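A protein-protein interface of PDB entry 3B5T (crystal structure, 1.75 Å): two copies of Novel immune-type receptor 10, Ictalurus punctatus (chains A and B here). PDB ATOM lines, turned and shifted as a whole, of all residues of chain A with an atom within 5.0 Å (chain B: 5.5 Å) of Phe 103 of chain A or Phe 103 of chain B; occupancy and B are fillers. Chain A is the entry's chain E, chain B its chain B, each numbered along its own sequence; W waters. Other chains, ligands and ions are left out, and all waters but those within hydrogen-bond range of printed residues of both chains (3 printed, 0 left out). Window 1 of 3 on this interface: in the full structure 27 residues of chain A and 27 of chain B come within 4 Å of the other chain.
The side-chain hydroxyl (OH) of Tyr 35 of chain B lies within hydrogen-bond range of the backbone NH (N) of Ile 101 of chain A, 3.1 Å away. The backbone NH of Val 42 of chain B sits at hydrogen-bond distance from the backbone carbonyl oxygen of Lys 4 of chain A. The backbone NH (N) of Ile 101 of chain B lies within hydrogen-bond range of the side-chain hydroxyl (OH) of Tyr 35 of chain A, at 3.0 Å.
N of Tyr 35 of chain B is in hydrogen-bond range of O of Phe 92 of chain B (2.7 Å). O of Phe 92 of chain A is in hydrogen-bond range of N of Tyr 35 of chain A (2.8 Å). N of Cys 93 of chain A lies within hydrogen-bond range of O of Ser 105 of chain A, at 2.8 Å.
CG1 of Val 42 of chain A touches CB of Phe 103 of chain B, 3.5 Å away. Phe 92 of chain B touches Pro 43 of chain A (CD1 to CD, 3.6 Å). Phe 103 of chain B touches Pro 43 of chain A. Phe 92 of chain A touches Pro 43 of chain B. Ile 101 of chain A touches Ile 101 of chain B (CG2 to CD1, 3.7 Å). Phe 103 of chain A touches Val 42 of chain B. Phe 103 of chain A touches Pro 43 of chain B (CD2 to O, 3.5 Å). Phe 103 of chain A touches Phe 103 of chain B. CG2 of Val 42 of chain B touches C of Ser 105 of chain A, at 3.9 Å.
Of the printed residues of chain B, Phe 103 of chain A touches Val 42 (3.2 Å), Pro 43 (3.5 Å) and Phe 103 (3.9 Å). Of the printed residues of chain A, Ile 101 of chain B touches Tyr 35 (3.0 Å) and Ile 101 (3.7 Å). Of the printed residues of chain B, Ser 105 of chain A touches Val 42. Printed residues of chain B within 4 Å of Phe 92 of chain A: Pro 43 (3.5 Å). Printed residues of chain A within 4 Å of Val 42 of chain B: Lys 4 (2.9 Å), Phe 103 (3.2 Å) and Ser 105 (3.9 Å). Printed residues of chain B within 4 Å of Tyr 35 of chain A: Ile 101. Lys 102 of chain B touches none of the printed residues of chain A. Gly 94 of chain B touches none of the printed residues of chain A.
Printed residues of chain B that touch a printed residue of chain A: Tyr 35, Val 42, Pro 43, Phe 92, Ile 101 and Phe 103. Of the 13 printed residues of chain A, 8 touch a printed residue of chain B. Printed residues of chain A that touch a printed residue of chain B: Lys 4, Tyr 35, Val 42, Pro 43, Phe 92, Ile 101, Phe 103 and Ser 105. Hydrophobic or aromatic side chains of chain A within 4 Å of the printed part of chain B: Tyr 35, Val 42, Pro 43, Phe 92, Ile 101 and Phe 103.
Val 42 of chain A touches Phe 103 of chain B, and with the chains exchanged Phe 103 of chain A touches Val 42 of chain B. Pro 43 of chain A touches Phe 92 of chain B, and with the chains exchanged Phe 92 of chain A touches Pro 43 of chain B. Ile 101 of chain A touches its own counterpart, Ile 101 of chain B. Ser 105 of chain A touches Val 42 of chain B, but with the chains exchanged Val 42 of chain A does not touch Ser 105 of chain B (4.1 Å). Positions printed for both chains: 35, 42, 43, 92, 93, 94, 95, 101, 102, 103, 104 and 105. Of the 12 pairs that touch across the chains among the printed residues, 10 have their exchanged pair printed and touching as well.
Water W1 lies within hydrogen-bond range of the backbone carbonyl oxygen (O) of Pro 43 of chain B and the backbone NH (N) of Phe 103 of chain A. Water W2 bridges the backbone carbonyl oxygen of Pro 43 of chain A and the backbone NH of Phe 103 of chain B. Water W3 lies within hydrogen-bond range of O of Val 42 of chain B, N of Lys 4 of chain A and NE2 of Gln 44 of chain B.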
ATOM      1  N   LYS A   4      12.801   9.540 -22.725  1.00  0.00           N
ATOM      2  CA  LYS A   4      13.157   9.300 -21.323  1.00  0.00           C
ATOM      3  C   LYS A   4      11.942   8.931 -20.492  1.00  0.00           C
ATOM      4  O   LYS A   4      10.839   9.417 -20.729  1.00  0.00           O
ATOM      5  CB  LYS A   4      13.858  10.508 -20.692  1.00  0.00           C
ATOM      6  CG  LYS A   4      15.292  10.766 -21.175  1.00  0.00           C
ATOM      7  CD  LYS A   4      15.354  11.890 -22.191  1.00  0.00           C
ATOM      8  CE  LYS A   4      16.784  12.107 -22.721  1.00  0.00           C
ATOM      9  NZ  LYS A   4      17.264  10.984 -23.576  1.00  0.00           N
ATOM     10  N   TYR A  35       8.422  22.674 -14.953  1.00  0.00           N
ATOM     11  CA  TYR A  35       7.022  22.803 -15.325  1.00  0.00           C
ATOM     12  C   TYR A  35       6.259  21.831 -14.465  1.00  0.00           C
ATOM     13  O   TYR A  35       6.678  20.688 -14.296  1.00  0.00           O
ATOM     14  CB  TYR A  35       6.844  22.493 -16.836  1.00  0.00           C
ATOM     15  CG  TYR A  35       7.539  23.541 -17.657  1.00  0.00           C
ATOM     16  CD1 TYR A  35       6.827  24.625 -18.185  1.00  0.00           C
ATOM     17  CD2 TYR A  35       8.919  23.493 -17.851  1.00  0.00           C
ATOM     18  CE1 TYR A  35       7.474  25.638 -18.895  1.00  0.00           C
ATOM     19  CE2 TYR A  35       9.577  24.498 -18.561  1.00  0.00           C
ATOM     20  CZ  TYR A  35       8.849  25.560 -19.084  1.00  0.00           C
ATOM     21  OH  TYR A  35       9.501  26.547 -19.788  1.00  0.00           O
ATOM     22  N   VAL A  42      -3.444  21.410 -17.840  1.00  0.00           N
ATOM     23  CA  VAL A  42      -2.390  21.834 -18.764  1.00  0.00           C
ATOM     24  C   VAL A  42      -1.117  22.126 -17.953  1.00  0.00           C
ATOM     25  O   VAL A  42      -1.211  22.703 -16.876  1.00  0.00           O
ATOM     26  CB  VAL A  42      -2.858  23.058 -19.586  1.00  0.00           C
ATOM     27  CG1 VAL A  42      -1.771  23.530 -20.543  1.00  0.00           C
ATOM     28  CG2 VAL A  42      -4.143  22.704 -20.341  1.00  0.00           C
ATOM     29  N   PRO A  43       0.071  21.676 -18.427  1.00  0.00           N
ATOM     30  CA  PRO A  43       1.300  22.006 -17.682  1.00  0.00           C
ATOM     31  C   PRO A  43       1.528  23.511 -17.579  1.00  0.00           C
ATOM     32  O   PRO A  43       1.138  24.263 -18.470  1.00  0.00           O
ATOM     33  CB  PRO A  43       2.417  21.374 -18.533  1.00  0.00           C
ATOM     34  CG  PRO A  43       1.722  20.272 -19.270  1.00  0.00           C
ATOM     35  CD  PRO A  43       0.363  20.836 -19.596  1.00  0.00           C
ATOM     36  N   PHE A  92       8.219  18.482 -15.116  1.00  0.00           N
ATOM     37  CA  PHE A  92       9.134  18.316 -16.264  1.00  0.00           C
ATOM     38  C   PHE A  92      10.204  19.400 -16.256  1.00  0.00           C
ATOM     39  O   PHE A  92       9.897  20.575 -16.032  1.00  0.00           O
ATOM     40  CB  PHE A  92       8.385  18.377 -17.610  1.00  0.00           C
ATOM     41  CG  PHE A  92       7.088  17.600 -17.643  1.00  0.00           C
ATOM     42  CD1 PHE A  92       7.046  16.219 -17.374  1.00  0.00           C
ATOM     43  CD2 PHE A  92       5.902  18.247 -17.987  1.00  0.00           C
ATOM     44  CE1 PHE A  92       5.830  15.509 -17.426  1.00  0.00           C
ATOM     45  CE2 PHE A  92       4.689  17.548 -18.025  1.00  0.00           C
ATOM     46  CZ  PHE A  92       4.645  16.188 -17.750  1.00  0.00           C
ATOM     47  N   CYS A  93      11.453  18.999 -16.502  1.00  0.00           N
ATOM     48  CA  CYS A  93      12.569  19.927 -16.571  1.00  0.00           C
ATOM     49  C   CYS A  93      12.950  20.076 -18.034  1.00  0.00           C
ATOM     50  O   CYS A  93      13.242  19.078 -18.717  1.00  0.00           O
ATOM     51  CB  CYS A  93      13.763  19.427 -15.762  1.00  0.00           C
ATOM     52  SG  CYS A  93      15.086  20.629 -15.663  1.00  0.00           S
ATOM     53  N   GLY A  94      12.911  21.310 -18.511  1.00  0.00           N
ATOM     54  CA  GLY A  94      13.192  21.564 -19.914  1.00  0.00           C
ATOM     55  C   GLY A  94      13.897  22.861 -20.216  1.00  0.00           C
ATOM     56  O   GLY A  94      13.775  23.871 -19.487  1.00  0.00           O
ATOM     57  N   GLU A  95      14.595  22.845 -21.348  1.00  0.00           N
ATOM     58  CA  GLU A  95      15.330  24.006 -21.800  1.00  0.00           C
ATOM     59  C   GLU A  95      14.794  24.463 -23.152  1.00  0.00           C
ATOM     60  O   GLU A  95      14.735  23.657 -24.095  1.00  0.00           O
ATOM     61  CB  GLU A  95      16.827  23.684 -21.916  1.00  0.00           C
ATOM     62  CG  GLU A  95      17.706  24.901 -22.256  1.00  0.00           C
ATOM     63  CD  GLU A  95      19.148  24.533 -22.618  1.00  0.00           C
ATOM     64  OE1 GLU A  95      19.553  23.366 -22.402  1.00  0.00           O
ATOM     65  OE2 GLU A  95      19.875  25.429 -23.113  1.00  0.00           O
ATOM     66  N   ILE A 101      10.837  23.561 -26.914  1.00  0.00           N
ATOM     67  CA  ILE A 101      11.505  23.212 -25.653  1.00  0.00           C
ATOM     68  C   ILE A 101      11.902  21.737 -25.693  1.00  0.00           C
ATOM     69  O   ILE A 101      11.193  20.886 -26.268  1.00  0.00           O
ATOM     70  CB  ILE A 101      10.592  23.530 -24.430  1.00  0.00           C
ATOM     71  CG1 ILE A 101      11.302  23.232 -23.092  1.00  0.00           C
ATOM     72  CG2 ILE A 101       9.301  22.758 -24.535  1.00  0.00           C
ATOM     73  CD1 ILE A 101      10.645  23.923 -21.887  1.00  0.00           C
ATOM     74  N   LYS A 102      13.041  21.433 -25.082  1.00  0.00           N
ATOM     75  CA  LYS A 102      13.509  20.074 -24.958  1.00  0.00           C
ATOM     76  C   LYS A 102      13.471  19.679 -23.490  1.00  0.00           C
ATOM     77  O   LYS A 102      14.149  20.293 -22.689  1.00  0.00           O
ATOM     78  CB  LYS A 102      14.952  20.005 -25.442  1.00  0.00           C
ATOM     79  CG  LYS A 102      15.306  18.692 -26.095  1.00  0.00           C
ATOM     80  CD  LYS A 102      16.134  17.787 -25.190  1.00  0.00           C
ATOM     81  CE  LYS A 102      16.958  16.796 -26.012  1.00  0.00           C
ATOM     82  NZ  LYS A 102      16.126  15.807 -26.784  1.00  0.00           N
ATOM     83  N   PHE A 103      12.689  18.665 -23.148  1.00  0.00           N
ATOM     84  CA  PHE A 103      12.609  18.198 -21.761  1.00  0.00           C
ATOM     85  C   PHE A 103      13.619  17.085 -21.565  1.00  0.00           C
ATOM     86  O   PHE A 103      13.684  16.152 -22.383  1.00  0.00           O
ATOM     87  CB  PHE A 103      11.206  17.702 -21.422  1.00  0.00           C
ATOM     88  CG  PHE A 103      10.157  18.766 -21.457  1.00  0.00           C
ATOM     89  CD1 PHE A 103      10.099  19.744 -20.467  1.00  0.00           C
ATOM     90  CD2 PHE A 103       9.188  18.770 -22.463  1.00  0.00           C
ATOM     91  CE1 PHE A 103       9.110  20.735 -20.505  1.00  0.00           C
ATOM     92  CE2 PHE A 103       8.201  19.738 -22.500  1.00  0.00           C
ATOM     93  CZ  PHE A 103       8.158  20.727 -21.514  1.00  0.00           C
ATOM     94  N   THR A 104      14.416  17.185 -20.507  1.00  0.00           N
ATOM     95  CA  THR A 104      15.504  16.236 -20.265  1.00  0.00           C
ATOM     96  C   THR A 104      15.215  15.256 -19.146  1.00  0.00           C
ATOM     97  O   THR A 104      15.837  14.184 -19.065  1.00  0.00           O
ATOM     98  CB  THR A 104      16.814  16.950 -19.978  1.00  0.00           C
ATOM     99  OG1 THR A 104      16.702  17.746 -18.785  1.00  0.00           O
ATOM    100  CG2 THR A 104      17.179  17.851 -21.144  1.00  0.00           C
ATOM    101  N   SER A 105      14.293  15.644 -18.266  1.00  0.00           N
ATOM    102  CA  SER A 105      13.860  14.773 -17.184  1.00  0.00           C
ATOM    103  C   SER A 105      12.484  15.163 -16.681  1.00  0.00           C
ATOM    104  O   SER A 105      12.002  16.273 -16.933  1.00  0.00           O
ATOM    105  CB  SER A 105      14.867  14.813 -16.018  1.00  0.00           C
ATOM    106  OG  SER A 105      14.909  16.082 -15.394  1.00  0.00           O
ATOM    107  N   TYR B  35       3.297  18.959 -28.414  1.00  0.00           N
ATOM    108  CA  TYR B  35       4.146  18.085 -27.601  1.00  0.00           C
ATOM    109  C   TYR B  35       3.353  16.843 -27.317  1.00  0.00           C
ATOM    110  O   TYR B  35       2.167  16.932 -26.976  1.00  0.00           O
ATOM    111  CB  TYR B  35       4.578  18.830 -26.301  1.00  0.00           C
ATOM    112  CG  TYR B  35       5.478  19.976 -26.685  1.00  0.00           C
ATOM    113  CD1 TYR B  35       6.863  19.849 -26.631  1.00  0.00           C
ATOM    114  CD2 TYR B  35       4.949  21.169 -27.168  1.00  0.00           C
ATOM    115  CE1 TYR B  35       7.711  20.887 -27.050  1.00  0.00           C
ATOM    116  CE2 TYR B  35       5.778  22.221 -27.590  1.00  0.00           C
ATOM    117  CZ  TYR B  35       7.157  22.078 -27.521  1.00  0.00           C
ATOM    118  OH  TYR B  35       7.974  23.108 -27.953  1.00  0.00           O
ATOM    119  N   VAL B  42       8.750  11.406 -20.541  1.00  0.00           N
ATOM    120  CA  VAL B  42       8.935  12.842 -20.655  1.00  0.00           C
ATOM    121  C   VAL B  42       8.249  13.308 -21.957  1.00  0.00           C
ATOM    122  O   VAL B  42       8.319  12.602 -22.971  1.00  0.00           O
ATOM    123  CB  VAL B  42      10.447  13.163 -20.657  1.00  0.00           C
ATOM    124  CG1 VAL B  42      10.698  14.606 -20.838  1.00  0.00           C
ATOM    125  CG2 VAL B  42      11.108  12.670 -19.333  1.00  0.00           C
ATOM    126  N   PRO B  43       7.530  14.451 -21.926  1.00  0.00           N
ATOM    127  CA  PRO B  43       6.933  14.947 -23.172  1.00  0.00           C
ATOM    128  C   PRO B  43       7.999  15.221 -24.229  1.00  0.00           C
ATOM    129  O   PRO B  43       9.141  15.603 -23.896  1.00  0.00           O
ATOM    130  CB  PRO B  43       6.292  16.277 -22.748  1.00  0.00           C
ATOM    131  CG  PRO B  43       6.058  16.139 -21.258  1.00  0.00           C
ATOM    132  CD  PRO B  43       7.214  15.320 -20.773  1.00  0.00           C
ATOM    133  N   GLN B  44       7.614  15.060 -25.498  1.00  0.00           N
ATOM    134  CA  GLN B  44       8.514  15.320 -26.599  1.00  0.00           C
ATOM    135  C   GLN B  44       7.894  16.277 -27.606  1.00  0.00           C
ATOM    136  O   GLN B  44       6.737  16.105 -27.957  1.00  0.00           O
ATOM    137  CB  GLN B  44       8.793  14.033 -27.356  1.00  0.00           C
ATOM    138  CG  GLN B  44      10.134  14.037 -28.029  1.00  0.00           C
ATOM    139  CD  GLN B  44      11.098  13.049 -27.406  1.00  0.00           C
ATOM    140  OE1 GLN B  44      11.796  12.329 -28.121  1.00  0.00           O
ATOM    141  NE2 GLN B  44      11.122  12.982 -26.072  1.00  0.00           N
ATOM    142  N   PHE B  92       0.089  18.422 -25.759  1.00  0.00           N
ATOM    143  CA  PHE B  92       0.039  19.799 -25.295  1.00  0.00           C
ATOM    144  C   PHE B  92       0.447  20.730 -26.411  1.00  0.00           C
ATOM    145  O   PHE B  92       1.425  20.467 -27.118  1.00  0.00           O
ATOM    146  CB  PHE B  92       1.018  20.022 -24.135  1.00  0.00           C
ATOM    147  CG  PHE B  92       0.978  18.936 -23.063  1.00  0.00           C
ATOM    148  CD1 PHE B  92      -0.193  18.627 -22.394  1.00  0.00           C
ATOM    149  CD2 PHE B  92       2.147  18.246 -22.717  1.00  0.00           C
ATOM    150  CE1 PHE B  92      -0.211  17.633 -21.398  1.00  0.00           C
ATOM    151  CE2 PHE B  92       2.127  17.243 -21.720  1.00  0.00           C
ATOM    152  CZ  PHE B  92       0.971  16.951 -21.072  1.00  0.00           C
ATOM    153  N   CYS B  93      -0.277  21.837 -26.534  1.00  0.00           N
ATOM    154  CA  CYS B  93       0.041  22.857 -27.520  1.00  0.00           C
ATOM    155  C   CYS B  93       0.656  24.033 -26.772  1.00  0.00           C
ATOM    156  O   CYS B  93       0.035  24.588 -25.852  1.00  0.00           O
ATOM    157  CB  CYS B  93      -1.236  23.288 -28.228  1.00  0.00           C
ATOM    158  SG  CYS B  93      -0.927  24.461 -29.560  1.00  0.00           S
ATOM    159  N   GLY B  94       1.877  24.396 -27.146  1.00  0.00           N
ATOM    160  CA  GLY B  94       2.614  25.447 -26.445  1.00  0.00           C
ATOM    161  C   GLY B  94       3.344  26.401 -27.361  1.00  0.00           C
ATOM    162  O   GLY B  94       3.792  26.019 -28.456  1.00  0.00           O
ATOM    163  N   GLU B  95       3.493  27.633 -26.884  1.00  0.00           N
ATOM    164  CA  GLU B  95       4.244  28.666 -27.583  1.00  0.00           C
ATOM    165  C   GLU B  95       5.430  29.127 -26.740  1.00  0.00           C
ATOM    166  O   GLU B  95       5.263  29.572 -25.585  1.00  0.00           O
ATOM    167  CB  GLU B  95       3.334  29.855 -27.923  1.00  0.00           C
ATOM    168  CG  GLU B  95       4.072  30.980 -28.585  1.00  0.00           C
ATOM    169  CD  GLU B  95       3.182  32.199 -28.912  1.00  0.00           C
ATOM    170  OE1 GLU B  95       1.963  32.165 -28.667  1.00  0.00           O
ATOM    171  OE2 GLU B  95       3.736  33.188 -29.432  1.00  0.00           O
ATOM    172  N   ILE B 101       8.242  28.183 -22.033  1.00  0.00           N
ATOM    173  CA  ILE B 101       7.132  27.889 -22.925  1.00  0.00           C
ATOM    174  C   ILE B 101       5.807  28.110 -22.198  1.00  0.00           C
ATOM    175  O   ILE B 101       5.679  27.871 -20.984  1.00  0.00           O
ATOM    176  CB  ILE B 101       7.210  26.453 -23.480  1.00  0.00           C
ATOM    177  CG1 ILE B 101       6.177  26.244 -24.597  1.00  0.00           C
ATOM    178  CG2 ILE B 101       7.183  25.381 -22.335  1.00  0.00           C
ATOM    179  CD1 ILE B 101       6.438  24.975 -25.464  1.00  0.00           C
ATOM    180  N   LYS B 102       4.813  28.594 -22.918  1.00  0.00           N
ATOM    181  CA  LYS B 102       3.514  28.576 -22.312  1.00  0.00           C
ATOM    182  C   LYS B 102       2.527  27.700 -23.072  1.00  0.00           C
ATOM    183  O   LYS B 102       2.329  27.865 -24.280  1.00  0.00           O
ATOM    184  CB  LYS B 102       3.041  29.982 -22.011  1.00  0.00           C
ATOM    185  CG  LYS B 102       2.273  30.616 -23.022  1.00  0.00           C
ATOM    186  CD  LYS B 102       0.884  30.863 -22.512  1.00  0.00           C
ATOM    187  CE  LYS B 102       0.244  31.948 -23.347  1.00  0.00           C
ATOM    188  NZ  LYS B 102       0.648  31.831 -24.780  1.00  0.00           N
ATOM    189  N   PHE B 103       1.934  26.758 -22.347  1.00  0.00           N
ATOM    190  CA  PHE B 103       1.023  25.810 -22.944  1.00  0.00           C
ATOM    191  C   PHE B 103      -0.366  26.374 -22.861  1.00  0.00           C
ATOM    192  O   PHE B 103      -0.802  26.819 -21.794  1.00  0.00           O
ATOM    193  CB  PHE B 103       1.094  24.463 -22.228  1.00  0.00           C
ATOM    194  CG  PHE B 103       2.395  23.762 -22.409  1.00  0.00           C
ATOM    195  CD1 PHE B 103       2.683  23.120 -23.613  1.00  0.00           C
ATOM    196  CD2 PHE B 103       3.339  23.738 -21.387  1.00  0.00           C
ATOM    197  CE1 PHE B 103       3.902  22.468 -23.792  1.00  0.00           C
ATOM    198  CE2 PHE B 103       4.551  23.085 -21.544  1.00  0.00           C
ATOM    199  CZ  PHE B 103       4.839  22.437 -22.764  1.00  0.00           C
ATOM    200  N   THR B 104      -1.064  26.370 -23.982  1.00  0.00           N
ATOM    201  CA  THR B 104      -2.363  27.017 -24.034  1.00  0.00           C
ATOM    202  C   THR B 104      -3.514  26.041 -24.102  1.00  0.00           C
ATOM    203  O   THR B 104      -4.667  26.409 -23.845  1.00  0.00           O
ATOM    204  CB  THR B 104      -2.432  27.987 -25.187  1.00  0.00           C
ATOM    205  OG1 THR B 104      -2.277  27.262 -26.406  1.00  0.00           O
ATOM    206  CG2 THR B 104      -1.292  29.010 -25.038  1.00  0.00           C
ATOM    207  N   SER B 105      -3.196  24.801 -24.454  1.00  0.00           N
ATOM    208  CA  SER B 105      -4.193  23.769 -24.572  1.00  0.00           C
ATOM    209  C   SER B 105      -3.563  22.397 -24.431  1.00  0.00           C
ATOM    210  O   SER B 105      -2.385  22.210 -24.711  1.00  0.00           O
ATOM    211  CB  SER B 105      -4.854  23.836 -25.944  1.00  0.00           C
ATOM    212  OG  SER B 105      -6.089  23.170 -25.866  1.00  0.00           O
HETATM  213  O   HOH W   1      11.530  16.519 -24.735  1.00  0.00           O
HETATM  214  O   HOH W   2       1.113  26.826 -19.374  1.00  0.00           O
HETATM  215  O   HOH W   3      10.275  10.926 -23.876  1.00  0.00           O
